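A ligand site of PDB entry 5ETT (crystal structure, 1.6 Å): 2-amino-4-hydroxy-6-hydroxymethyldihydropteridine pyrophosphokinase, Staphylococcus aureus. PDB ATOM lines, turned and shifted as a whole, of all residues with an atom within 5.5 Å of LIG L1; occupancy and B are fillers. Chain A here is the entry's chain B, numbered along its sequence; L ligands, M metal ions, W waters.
O of Gly 93 is in hydrogen-bond range of NE of Arg 95.
OG1 of Thr 52 lies within hydrogen-bond range of NE2 of Gln 54, at 3.1 Å.
O of Pro 55 is in hydrogen-bond range of ND2 of Asn 14, 3.0 Å away.
The backbone NH (N) of Thr 46 is in hydrogen-bond range of the backbone carbonyl oxygen (O) of Phe 57 (2.9 Å).
The backbone carbonyl oxygen (O) of Trp 92 is in hydrogen-bond range of the side-chain hydroxyl (OH) of Tyr 51, 2.7 Å away.
The side-chain amide nitrogen (ND2) of Asn 59 sits at hydrogen-bond distance from the backbone carbonyl oxygen (O) of Leu 11 (3.1 Å).
OG1 of Thr 46 is in hydrogen-bond range of OD1 of Asn 59 (2.6 Å).
OD1 of Asn 14 is in hydrogen-bond range of N of Arg 95 (2.9 Å).
A nitrogen (N6) of LIG L1 lies within hydrogen-bond range of the backbone carbonyl oxygen of Ala 47 (2.9 Å).
NH1 of Arg 95 lies within salt-bridge range of O5 of LG2 L2, at 3.0 Å.
NH2 of Arg 124 is in salt-bridge range of O3 of LG2 L2.
The side-chain amide nitrogen of Asn 14 is in hydrogen-bond range of a nitrogen (N1) of LIG L1 (3.1 Å).
The side-chain hydroxyl (OG1) of Thr 46 sits at hydrogen-bond distance from a nitrogen (N6) of LIG L1 (2.9 Å).
A nitrogen (N2) of LIG L1 is in hydrogen-bond range of the backbone NH of Val 49 (3.1 Å).
The guanidinium group (NH2) of Arg 124 sits close to a sulfur (S1) of LIG L1, at 3.4 Å.
The backbone carbonyl oxygen (O) of Val 49 is in hydrogen-bond range of a nitrogen (N3) of LIG L1 (2.9 Å).
The side-chain amide nitrogen of Asn 59 lies within hydrogen-bond range of an oxygen (O1) of LIG L1 (2.9 Å).
Water W3 lies within hydrogen-bond range of N5 of LIG L1 (2.8 Å), O5 of LG2 L2 (2.8 Å) and NH1 of Arg 95 (3.1 Å).
Water W2 lies within hydrogen-bond range of O1 of LIG L1 (3.0 Å) and NH1 of Arg 95 (3.1 Å).
N1 of LIG L1 lies close to O of Gly 93 (3.4 Å).
N1 of LIG L1 sits close to N of Pro 94 (3.1 Å).
NH2 of Arg 95 sits close to F1 of LIG L1 (3.3 Å).
Pro 48 touches LIG L1.
CB of Tyr 51 touches C3 of LIG L1, at 3.6 Å.
CG of Gln 54 touches N1 of LIG L1, 3.6 Å away.
CD1 of Phe 57 touches N4 of LIG L1, at 3.4 Å.
Trp 92 touches LIG L1 (CE3 to F1, 3.3 Å).
Phe 126 touches LIG L1.
15 residues have an atom within 4 Å of LIG L1: Asn 14, Thr 46, Ala 47, Pro 48, Val 49, Tyr 51, Gln 54, Phe 57, Asn 59, Trp 92, Gly 93, Pro 94, Arg 95, Arg 124 and Phe 126.
The nearest printed residue that does not touch LIG L1 is Gly 12 (4.3 Å).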
ATOM      1  N   LEU A  11     -24.266  23.772 -20.947  1.00  0.00           N
ATOM      2  CA  LEU A  11     -23.585  23.909 -22.255  1.00  0.00           C
ATOM      3  C   LEU A  11     -22.103  23.847 -22.035  1.00  0.00           C
ATOM      4  O   LEU A  11     -21.598  24.372 -21.053  1.00  0.00           O
ATOM      5  CB  LEU A  11     -23.957  25.186 -22.987  1.00  0.00           C
ATOM      6  CG  LEU A  11     -25.249  25.213 -23.762  1.00  0.00           C
ATOM      7  CD1 LEU A  11     -26.429  25.061 -22.860  1.00  0.00           C
ATOM      8  CD2 LEU A  11     -25.364  26.489 -24.597  1.00  0.00           C
ATOM      9  N   GLY A  12     -21.432  23.215 -22.973  1.00  0.00           N
ATOM     10  CA  GLY A  12     -19.976  23.140 -22.915  1.00  0.00           C
ATOM     11  C   GLY A  12     -19.332  23.214 -24.309  1.00  0.00           C
ATOM     12  O   GLY A  12     -19.941  22.831 -25.300  1.00  0.00           O
ATOM     13  N   ASN A  14     -15.047  22.828 -25.903  1.00  0.00           N
ATOM     14  CA  ASN A  14     -13.575  22.749 -25.631  1.00  0.00           C
ATOM     15  C   ASN A  14     -12.753  22.641 -26.860  1.00  0.00           C
ATOM     16  O   ASN A  14     -11.633  22.116 -26.847  1.00  0.00           O
ATOM     17  CB  ASN A  14     -13.246  21.692 -24.572  1.00  0.00           C
ATOM     18  CG  ASN A  14     -13.279  20.312 -25.052  1.00  0.00           C
ATOM     19  OD1 ASN A  14     -14.040  19.971 -25.954  1.00  0.00           O
ATOM     20  ND2 ASN A  14     -12.398  19.468 -24.522  1.00  0.00           N
ATOM     21  N   THR A  46     -13.156  25.324 -17.138  1.00  0.00           N
ATOM     22  CA  THR A  46     -13.203  24.183 -16.271  1.00  0.00           C
ATOM     23  C   THR A  46     -12.297  23.105 -16.782  1.00  0.00           C
ATOM     24  O   THR A  46     -12.108  22.861 -18.013  1.00  0.00           O
ATOM     25  CB  THR A  46     -14.699  23.659 -16.131  1.00  0.00           C
ATOM     26  OG1 THR A  46     -15.121  23.083 -17.381  1.00  0.00           O
ATOM     27  CG2 THR A  46     -15.682  24.755 -15.681  1.00  0.00           C
ATOM     28  N   ALA A  47     -11.702  22.363 -15.856  1.00  0.00           N
ATOM     29  CA  ALA A  47     -10.898  21.239 -16.199  1.00  0.00           C
ATOM     30  C   ALA A  47     -11.750  20.040 -16.583  1.00  0.00           C
ATOM     31  O   ALA A  47     -12.737  19.738 -15.886  1.00  0.00           O
ATOM     32  CB  ALA A  47      -9.998  20.847 -15.012  1.00  0.00           C
ATOM     33  N   PRO A  48     -11.374  19.341 -17.642  1.00  0.00           N
ATOM     34  CA  PRO A  48     -12.152  18.154 -18.042  1.00  0.00           C
ATOM     35  C   PRO A  48     -12.231  17.129 -16.921  1.00  0.00           C
ATOM     36  O   PRO A  48     -11.179  16.861 -16.271  1.00  0.00           O
ATOM     37  CB  PRO A  48     -11.407  17.599 -19.208  1.00  0.00           C
ATOM     38  CG  PRO A  48     -10.643  18.683 -19.740  1.00  0.00           C
ATOM     39  CD  PRO A  48     -10.283  19.582 -18.579  1.00  0.00           C
ATOM     40  N   VAL A  49     -13.398  16.522 -16.743  1.00  0.00           N
ATOM     41  CA  VAL A  49     -13.567  15.403 -15.867  1.00  0.00           C
ATOM     42  C   VAL A  49     -14.079  14.179 -16.639  1.00  0.00           C
ATOM     43  O   VAL A  49     -14.736  14.277 -17.699  1.00  0.00           O
ATOM     44  CB  VAL A  49     -14.491  15.709 -14.683  1.00  0.00           C
ATOM     45  CG1 VAL A  49     -13.976  16.864 -13.872  1.00  0.00           C
ATOM     46  CG2 VAL A  49     -15.840  16.065 -15.139  1.00  0.00           C
ATOM     47  N   GLY A  50     -13.736  13.000 -16.092  1.00  0.00           N
ATOM     48  CA  GLY A  50     -14.216  11.743 -16.600  1.00  0.00           C
ATOM     49  C   GLY A  50     -13.484  11.091 -17.756  1.00  0.00           C
ATOM     50  O   GLY A  50     -13.987  10.204 -18.388  1.00  0.00           O
ATOM     51  N   TYR A  51     -12.299  11.595 -18.055  1.00  0.00           N
ATOM     52  CA  TYR A  51     -11.634  11.142 -19.285  1.00  0.00           C
ATOM     53  C   TYR A  51     -10.090  11.326 -19.091  1.00  0.00           C
ATOM     54  O   TYR A  51      -9.590  11.450 -18.002  1.00  0.00           O
ATOM     55  CB  TYR A  51     -12.206  11.830 -20.519  1.00  0.00           C
ATOM     56  CG  TYR A  51     -12.086  11.090 -21.832  1.00  0.00           C
ATOM     57  CD1 TYR A  51     -12.498   9.798 -21.997  1.00  0.00           C
ATOM     58  CD2 TYR A  51     -11.613  11.746 -22.962  1.00  0.00           C
ATOM     59  CE1 TYR A  51     -12.362   9.149 -23.239  1.00  0.00           C
ATOM     60  CE2 TYR A  51     -11.542  11.138 -24.179  1.00  0.00           C
ATOM     61  CZ  TYR A  51     -11.907   9.836 -24.333  1.00  0.00           C
ATOM     62  OH  TYR A  51     -11.773   9.222 -25.587  1.00  0.00           O
ATOM     63  N   THR A  52      -9.377  11.272 -20.180  1.00  0.00           N
ATOM     64  CA  THR A  52      -7.956  11.573 -20.191  1.00  0.00           C
ATOM     65  C   THR A  52      -7.726  13.087 -20.213  1.00  0.00           C
ATOM     66  O   THR A  52      -8.666  13.865 -20.339  1.00  0.00           O
ATOM     67  CB  THR A  52      -7.326  10.936 -21.455  1.00  0.00           C
ATOM     68  OG1 THR A  52      -8.102  11.251 -22.580  1.00  0.00           O
ATOM     69  CG2 THR A  52      -7.225   9.482 -21.312  1.00  0.00           C
ATOM     70  N   GLN A  54      -7.367  16.592 -21.598  1.00  0.00           N
ATOM     71  CA  GLN A  54      -8.052  17.163 -22.759  1.00  0.00           C
ATOM     72  C   GLN A  54      -8.053  18.676 -22.622  1.00  0.00           C
ATOM     73  O   GLN A  54      -7.792  19.174 -21.546  1.00  0.00           O
ATOM     74  CB  GLN A  54      -9.530  16.670 -22.844  1.00  0.00           C
ATOM     75  CG  GLN A  54      -9.666  15.168 -23.146  1.00  0.00           C
ATOM     76  CD  GLN A  54      -9.067  14.751 -24.488  1.00  0.00           C
ATOM     77  OE1 GLN A  54      -8.982  15.528 -25.425  1.00  0.00           O
ATOM     78  NE2 GLN A  54      -8.786  13.491 -24.595  1.00  0.00           N
ATOM     79  N   PRO A  55      -8.352  19.388 -23.675  1.00  0.00           N
ATOM     80  CA  PRO A  55      -8.414  20.848 -23.565  1.00  0.00           C
ATOM     81  C   PRO A  55      -9.493  21.321 -22.584  1.00  0.00           C
ATOM     82  O   PRO A  55     -10.568  20.680 -22.493  1.00  0.00           O
ATOM     83  CB  PRO A  55      -8.682  21.284 -25.006  1.00  0.00           C
ATOM     84  CG  PRO A  55      -8.680  20.102 -25.808  1.00  0.00           C
ATOM     85  CD  PRO A  55      -8.554  18.919 -25.034  1.00  0.00           C
ATOM     86  N   PHE A  57     -12.544  23.262 -20.926  1.00  0.00           N
ATOM     87  CA  PHE A  57     -13.863  23.625 -21.371  1.00  0.00           C
ATOM     88  C   PHE A  57     -14.186  25.061 -20.967  1.00  0.00           C
ATOM     89  O   PHE A  57     -13.779  25.530 -19.982  1.00  0.00           O
ATOM     90  CB  PHE A  57     -14.874  22.728 -20.684  1.00  0.00           C
ATOM     91  CG  PHE A  57     -15.020  21.393 -21.285  1.00  0.00           C
ATOM     92  CD1 PHE A  57     -14.224  20.355 -20.886  1.00  0.00           C
ATOM     93  CD2 PHE A  57     -15.977  21.154 -22.209  1.00  0.00           C
ATOM     94  CE1 PHE A  57     -14.400  19.098 -21.430  1.00  0.00           C
ATOM     95  CE2 PHE A  57     -16.138  19.916 -22.767  1.00  0.00           C
ATOM     96  CZ  PHE A  57     -15.359  18.898 -22.388  1.00  0.00           C
ATOM     97  N   ASN A  59     -17.858  26.327 -19.837  1.00  0.00           N
ATOM     98  CA  ASN A  59     -19.163  25.773 -19.468  1.00  0.00           C
ATOM     99  C   ASN A  59     -20.038  26.846 -18.929  1.00  0.00           C
ATOM    100  O   ASN A  59     -19.554  27.823 -18.283  1.00  0.00           O
ATOM    101  CB  ASN A  59     -19.066  24.717 -18.323  1.00  0.00           C
ATOM    102  CG  ASN A  59     -18.578  23.351 -18.791  1.00  0.00           C
ATOM    103  OD1 ASN A  59     -17.503  22.866 -18.414  1.00  0.00           O
ATOM    104  ND2 ASN A  59     -19.414  22.682 -19.623  1.00  0.00           N
ATOM    105  N   TRP A  92     -14.520   9.268 -27.689  1.00  0.00           N
ATOM    106  CA  TRP A  92     -14.841  10.631 -27.224  1.00  0.00           C
ATOM    107  C   TRP A  92     -13.631  11.533 -27.453  1.00  0.00           C
ATOM    108  O   TRP A  92     -12.465  11.148 -27.339  1.00  0.00           O
ATOM    109  CB  TRP A  92     -15.250  10.673 -25.741  1.00  0.00           C
ATOM    110  CG  TRP A  92     -16.384   9.782 -25.384  1.00  0.00           C
ATOM    111  CD1 TRP A  92     -17.369   9.245 -26.188  1.00  0.00           C
ATOM    112  CD2 TRP A  92     -16.669   9.338 -24.055  1.00  0.00           C
ATOM    113  NE1 TRP A  92     -18.253   8.481 -25.407  1.00  0.00           N
ATOM    114  CE2 TRP A  92     -17.835   8.528 -24.113  1.00  0.00           C
ATOM    115  CE3 TRP A  92     -16.038   9.545 -22.821  1.00  0.00           C
ATOM    116  CZ2 TRP A  92     -18.369   7.924 -22.951  1.00  0.00           C
ATOM    117  CZ3 TRP A  92     -16.566   8.962 -21.682  1.00  0.00           C
ATOM    118  CH2 TRP A  92     -17.709   8.157 -21.765  1.00  0.00           C
ATOM    119  N   GLY A  93     -13.936  12.795 -27.742  1.00  0.00           N
ATOM    120  CA  GLY A  93     -12.883  13.781 -27.815  1.00  0.00           C
ATOM    121  C   GLY A  93     -13.470  15.148 -27.671  1.00  0.00           C
ATOM    122  O   GLY A  93     -14.653  15.321 -27.304  1.00  0.00           O
ATOM    123  N   PRO A  94     -12.677  16.143 -28.049  1.00  0.00           N
ATOM    124  CA  PRO A  94     -13.092  17.511 -27.872  1.00  0.00           C
ATOM    125  C   PRO A  94     -14.365  17.789 -28.710  1.00  0.00           C
ATOM    126  O   PRO A  94     -14.621  17.144 -29.753  1.00  0.00           O
ATOM    127  CB  PRO A  94     -11.908  18.292 -28.409  1.00  0.00           C
ATOM    128  CG  PRO A  94     -10.747  17.354 -28.097  1.00  0.00           C
ATOM    129  CD  PRO A  94     -11.212  16.013 -28.360  1.00  0.00           C
ATOM    130  N   ARG A  95     -15.166  18.753 -28.282  1.00  0.00           N
ATOM    131  CA  ARG A  95     -16.438  19.003 -28.957  1.00  0.00           C
ATOM    132  C   ARG A  95     -16.681  20.488 -29.044  1.00  0.00           C
ATOM    133  O   ARG A  95     -16.446  21.285 -28.090  1.00  0.00           O
ATOM    134  CB  ARG A  95     -17.604  18.265 -28.284  1.00  0.00           C
ATOM    135  CG  ARG A  95     -17.915  18.644 -26.831  1.00  0.00           C
ATOM    136  CD  ARG A  95     -17.025  17.902 -25.820  1.00  0.00           C
ATOM    137  NE  ARG A  95     -16.980  16.505 -26.006  1.00  0.00           N
ATOM    138  CZ  ARG A  95     -17.876  15.660 -25.522  1.00  0.00           C
ATOM    139  NH1 ARG A  95     -18.852  16.101 -24.713  1.00  0.00           N
ATOM    140  NH2 ARG A  95     -17.815  14.406 -25.883  1.00  0.00           N
ATOM    141  N   ASP A  98     -21.698  20.943 -26.592  1.00  0.00           N
ATOM    142  CA  ASP A  98     -22.511  19.948 -25.906  1.00  0.00           C
ATOM    143  C   ASP A  98     -23.653  20.678 -25.216  1.00  0.00           C
ATOM    144  O   ASP A  98     -23.414  21.658 -24.480  1.00  0.00           O
ATOM    145  CB  ASP A  98     -21.642  19.224 -24.879  1.00  0.00           C
ATOM    146  CG  ASP A  98     -22.364  18.086 -24.158  1.00  0.00           C
ATOM    147  OD1 ASP A  98     -23.087  17.339 -24.842  1.00  0.00           O
ATOM    148  OD2 ASP A  98     -22.142  17.956 -22.880  1.00  0.00           O
ATOM    149  N   ARG A 124     -20.901  17.138 -10.335  1.00  0.00           N
ATOM    150  CA  ARG A 124     -20.113  17.883 -11.321  1.00  0.00           C
ATOM    151  C   ARG A 124     -20.060  19.384 -10.969  1.00  0.00           C
ATOM    152  O   ARG A 124     -21.012  20.039 -11.104  1.00  0.00           O
ATOM    153  CB  ARG A 124     -20.738  17.758 -12.696  1.00  0.00           C
ATOM    154  CG  ARG A 124     -20.320  16.500 -13.408  1.00  0.00           C
ATOM    155  CD  ARG A 124     -21.130  16.207 -14.659  1.00  0.00           C
ATOM    156  NE  ARG A 124     -20.505  15.148 -15.429  1.00  0.00           N
ATOM    157  CZ  ARG A 124     -20.830  14.848 -16.666  1.00  0.00           C
ATOM    158  NH1 ARG A 124     -21.829  15.487 -17.279  1.00  0.00           N
ATOM    159  NH2 ARG A 124     -20.170  13.883 -17.267  1.00  0.00           N
ATOM    160  N   PHE A 126     -18.598  21.633 -12.689  1.00  0.00           N
ATOM    161  CA  PHE A 126     -18.761  22.437 -13.909  1.00  0.00           C
ATOM    162  C   PHE A 126     -20.239  22.629 -14.261  1.00  0.00           C
ATOM    163  O   PHE A 126     -20.558  23.518 -15.094  1.00  0.00           O
ATOM    164  CB  PHE A 126     -18.013  21.857 -15.093  1.00  0.00           C
ATOM    165  CG  PHE A 126     -18.607  20.617 -15.705  1.00  0.00           C
ATOM    166  CD1 PHE A 126     -19.611  20.729 -16.601  1.00  0.00           C
ATOM    167  CD2 PHE A 126     -18.111  19.347 -15.414  1.00  0.00           C
ATOM    168  CE1 PHE A 126     -20.102  19.574 -17.270  1.00  0.00           C
ATOM    169  CE2 PHE A 126     -18.604  18.203 -16.026  1.00  0.00           C
ATOM    170  CZ  PHE A 126     -19.606  18.313 -16.936  1.00  0.00           C
HETATM  171  C1  LIG L   1     -13.070  15.795 -24.163  1.00  0.00           C
HETATM  172  C2  LIG L   1     -13.663  15.215 -21.927  1.00  0.00           C
HETATM  173  C3  LIG L   1     -14.466  14.556 -21.027  1.00  0.00           C
HETATM  174  C4  LIG L   1     -14.838  14.213 -23.711  1.00  0.00           C
HETATM  175  C5  LIG L   1     -13.864  15.067 -23.275  1.00  0.00           C
HETATM  176  C6  LIG L   1     -15.489  13.670 -21.403  1.00  0.00           C
HETATM  177  C7  LIG L   1     -17.638  17.915 -19.569  1.00  0.00           C
HETATM  178  C8  LIG L   1     -15.590  13.527 -22.776  1.00  0.00           C
HETATM  179  C9  LIG L   1     -16.663  17.355 -18.789  1.00  0.00           C
HETATM  180  C10 LIG L   1     -17.839  19.321 -19.632  1.00  0.00           C
HETATM  181  C11 LIG L   1     -15.924  19.312 -18.079  1.00  0.00           C
HETATM  182  C12 LIG L   1     -17.815  15.806 -19.789  1.00  0.00           C
HETATM  183  C13 LIG L   1     -16.517  13.044 -20.420  1.00  0.00           C
HETATM  184  N1  LIG L   1     -12.481  16.405 -24.953  1.00  0.00           N
HETATM  185  N2  LIG L   1     -15.768  18.020 -18.054  1.00  0.00           N
HETATM  186  N3  LIG L   1     -16.767  15.997 -18.901  1.00  0.00           N
HETATM  187  N4  LIG L   1     -16.909  19.965 -18.844  1.00  0.00           N
HETATM  188  N5  LIG L   1     -18.382  16.918 -20.176  1.00  0.00           N
HETATM  189  N6  LIG L   1     -15.182  20.186 -17.385  1.00  0.00           N
HETATM  190  O1  LIG L   1     -18.713  19.964 -20.287  1.00  0.00           O
HETATM  191  F1  LIG L   1     -16.525  12.724 -23.341  1.00  0.00           F
HETATM  192  S1  LIG L   1     -18.268  14.134 -20.132  1.00  0.00           S
HETATM  193  P1  LG2 L   2     -22.527  13.456 -20.374  1.00  0.00           P
HETATM  194  O1  LG2 L   2     -22.413  14.967 -20.098  1.00  0.00           O
HETATM  195  O2  LG2 L   2     -23.907  12.907 -20.513  1.00  0.00           O
HETATM  196  O3  LG2 L   2     -21.707  12.613 -19.406  1.00  0.00           O
HETATM  197  P2  LG2 L   2     -22.117  13.795 -23.232  1.00  0.00           P
HETATM  198  O4  LG2 L   2     -22.938  15.025 -22.949  1.00  0.00           O
HETATM  199  O5  LG2 L   2     -20.813  14.006 -23.943  1.00  0.00           O
HETATM  200  O6  LG2 L   2     -21.794  13.162 -21.799  1.00  0.00           O
HETATM  201  P3  LG2 L   2     -23.553  13.100 -25.692  1.00  0.00           P
HETATM  202  O7  LG2 L   2     -23.752  14.567 -25.726  1.00  0.00           O
HETATM  203  O8  LG2 L   2     -22.686  12.446 -26.713  1.00  0.00           O
HETATM  204  C1  LG2 L   2     -23.162  12.579 -23.999  1.00  0.00           C
HETATM  205  O9  LG2 L   2     -25.024  12.525 -25.969  1.00  0.00           O
HETATM  206  C2  LG2 L   2     -25.341  11.169 -26.143  1.00  0.00           C
HETATM  207  C3  LG2 L   2     -26.862  10.930 -25.927  1.00  0.00           C
HETATM  208  O10 LG2 L   2     -27.155  11.173 -24.570  1.00  0.00           O
HETATM  209  C4  LG2 L   2     -27.800  11.843 -26.658  1.00  0.00           C
HETATM  210  O11 LG2 L   2     -27.979  11.441 -27.998  1.00  0.00           O
HETATM  211  C5  LG2 L   2     -29.076  11.667 -25.865  1.00  0.00           C
HETATM  212  O12 LG2 L   2     -30.011  10.692 -26.439  1.00  0.00           O
HETATM  213  C6  LG2 L   2     -28.576  11.102 -24.574  1.00  0.00           C
HETATM  214  N1  LG2 L   2     -29.010  11.771 -23.319  1.00  0.00           N
HETATM  215  C7  LG2 L   2     -29.463  11.118 -22.178  1.00  0.00           C
HETATM  216  N2  LG2 L   2     -29.810  12.010 -21.225  1.00  0.00           N
HETATM  217  C8  LG2 L   2     -29.535  13.243 -21.798  1.00  0.00           C
HETATM  218  C9  LG2 L   2     -29.684  14.539 -21.249  1.00  0.00           C
HETATM  219  N3  LG2 L   2     -30.151  14.778 -19.976  1.00  0.00           N
HETATM  220  N4  LG2 L   2     -29.332  15.589 -22.031  1.00  0.00           N
HETATM  221  C10 LG2 L   2     -28.862  15.329 -23.257  1.00  0.00           C
HETATM  222  N5  LG2 L   2     -28.694  14.146 -23.904  1.00  0.00           N
HETATM  223  C11 LG2 L   2     -29.046  13.135 -23.083  1.00  0.00           C
HETATM  224 MG    MG M   1     -22.304  16.456 -21.482  1.00  0.00          MG
HETATM  225  O   HOH W   1     -21.374  17.733 -20.070  1.00  0.00           O
HETATM  226  O   HOH W   2     -19.210  18.599 -22.961  1.00  0.00           O
HETATM  227  O   HOH W   3     -20.303  15.902 -21.935  1.00  0.00           O
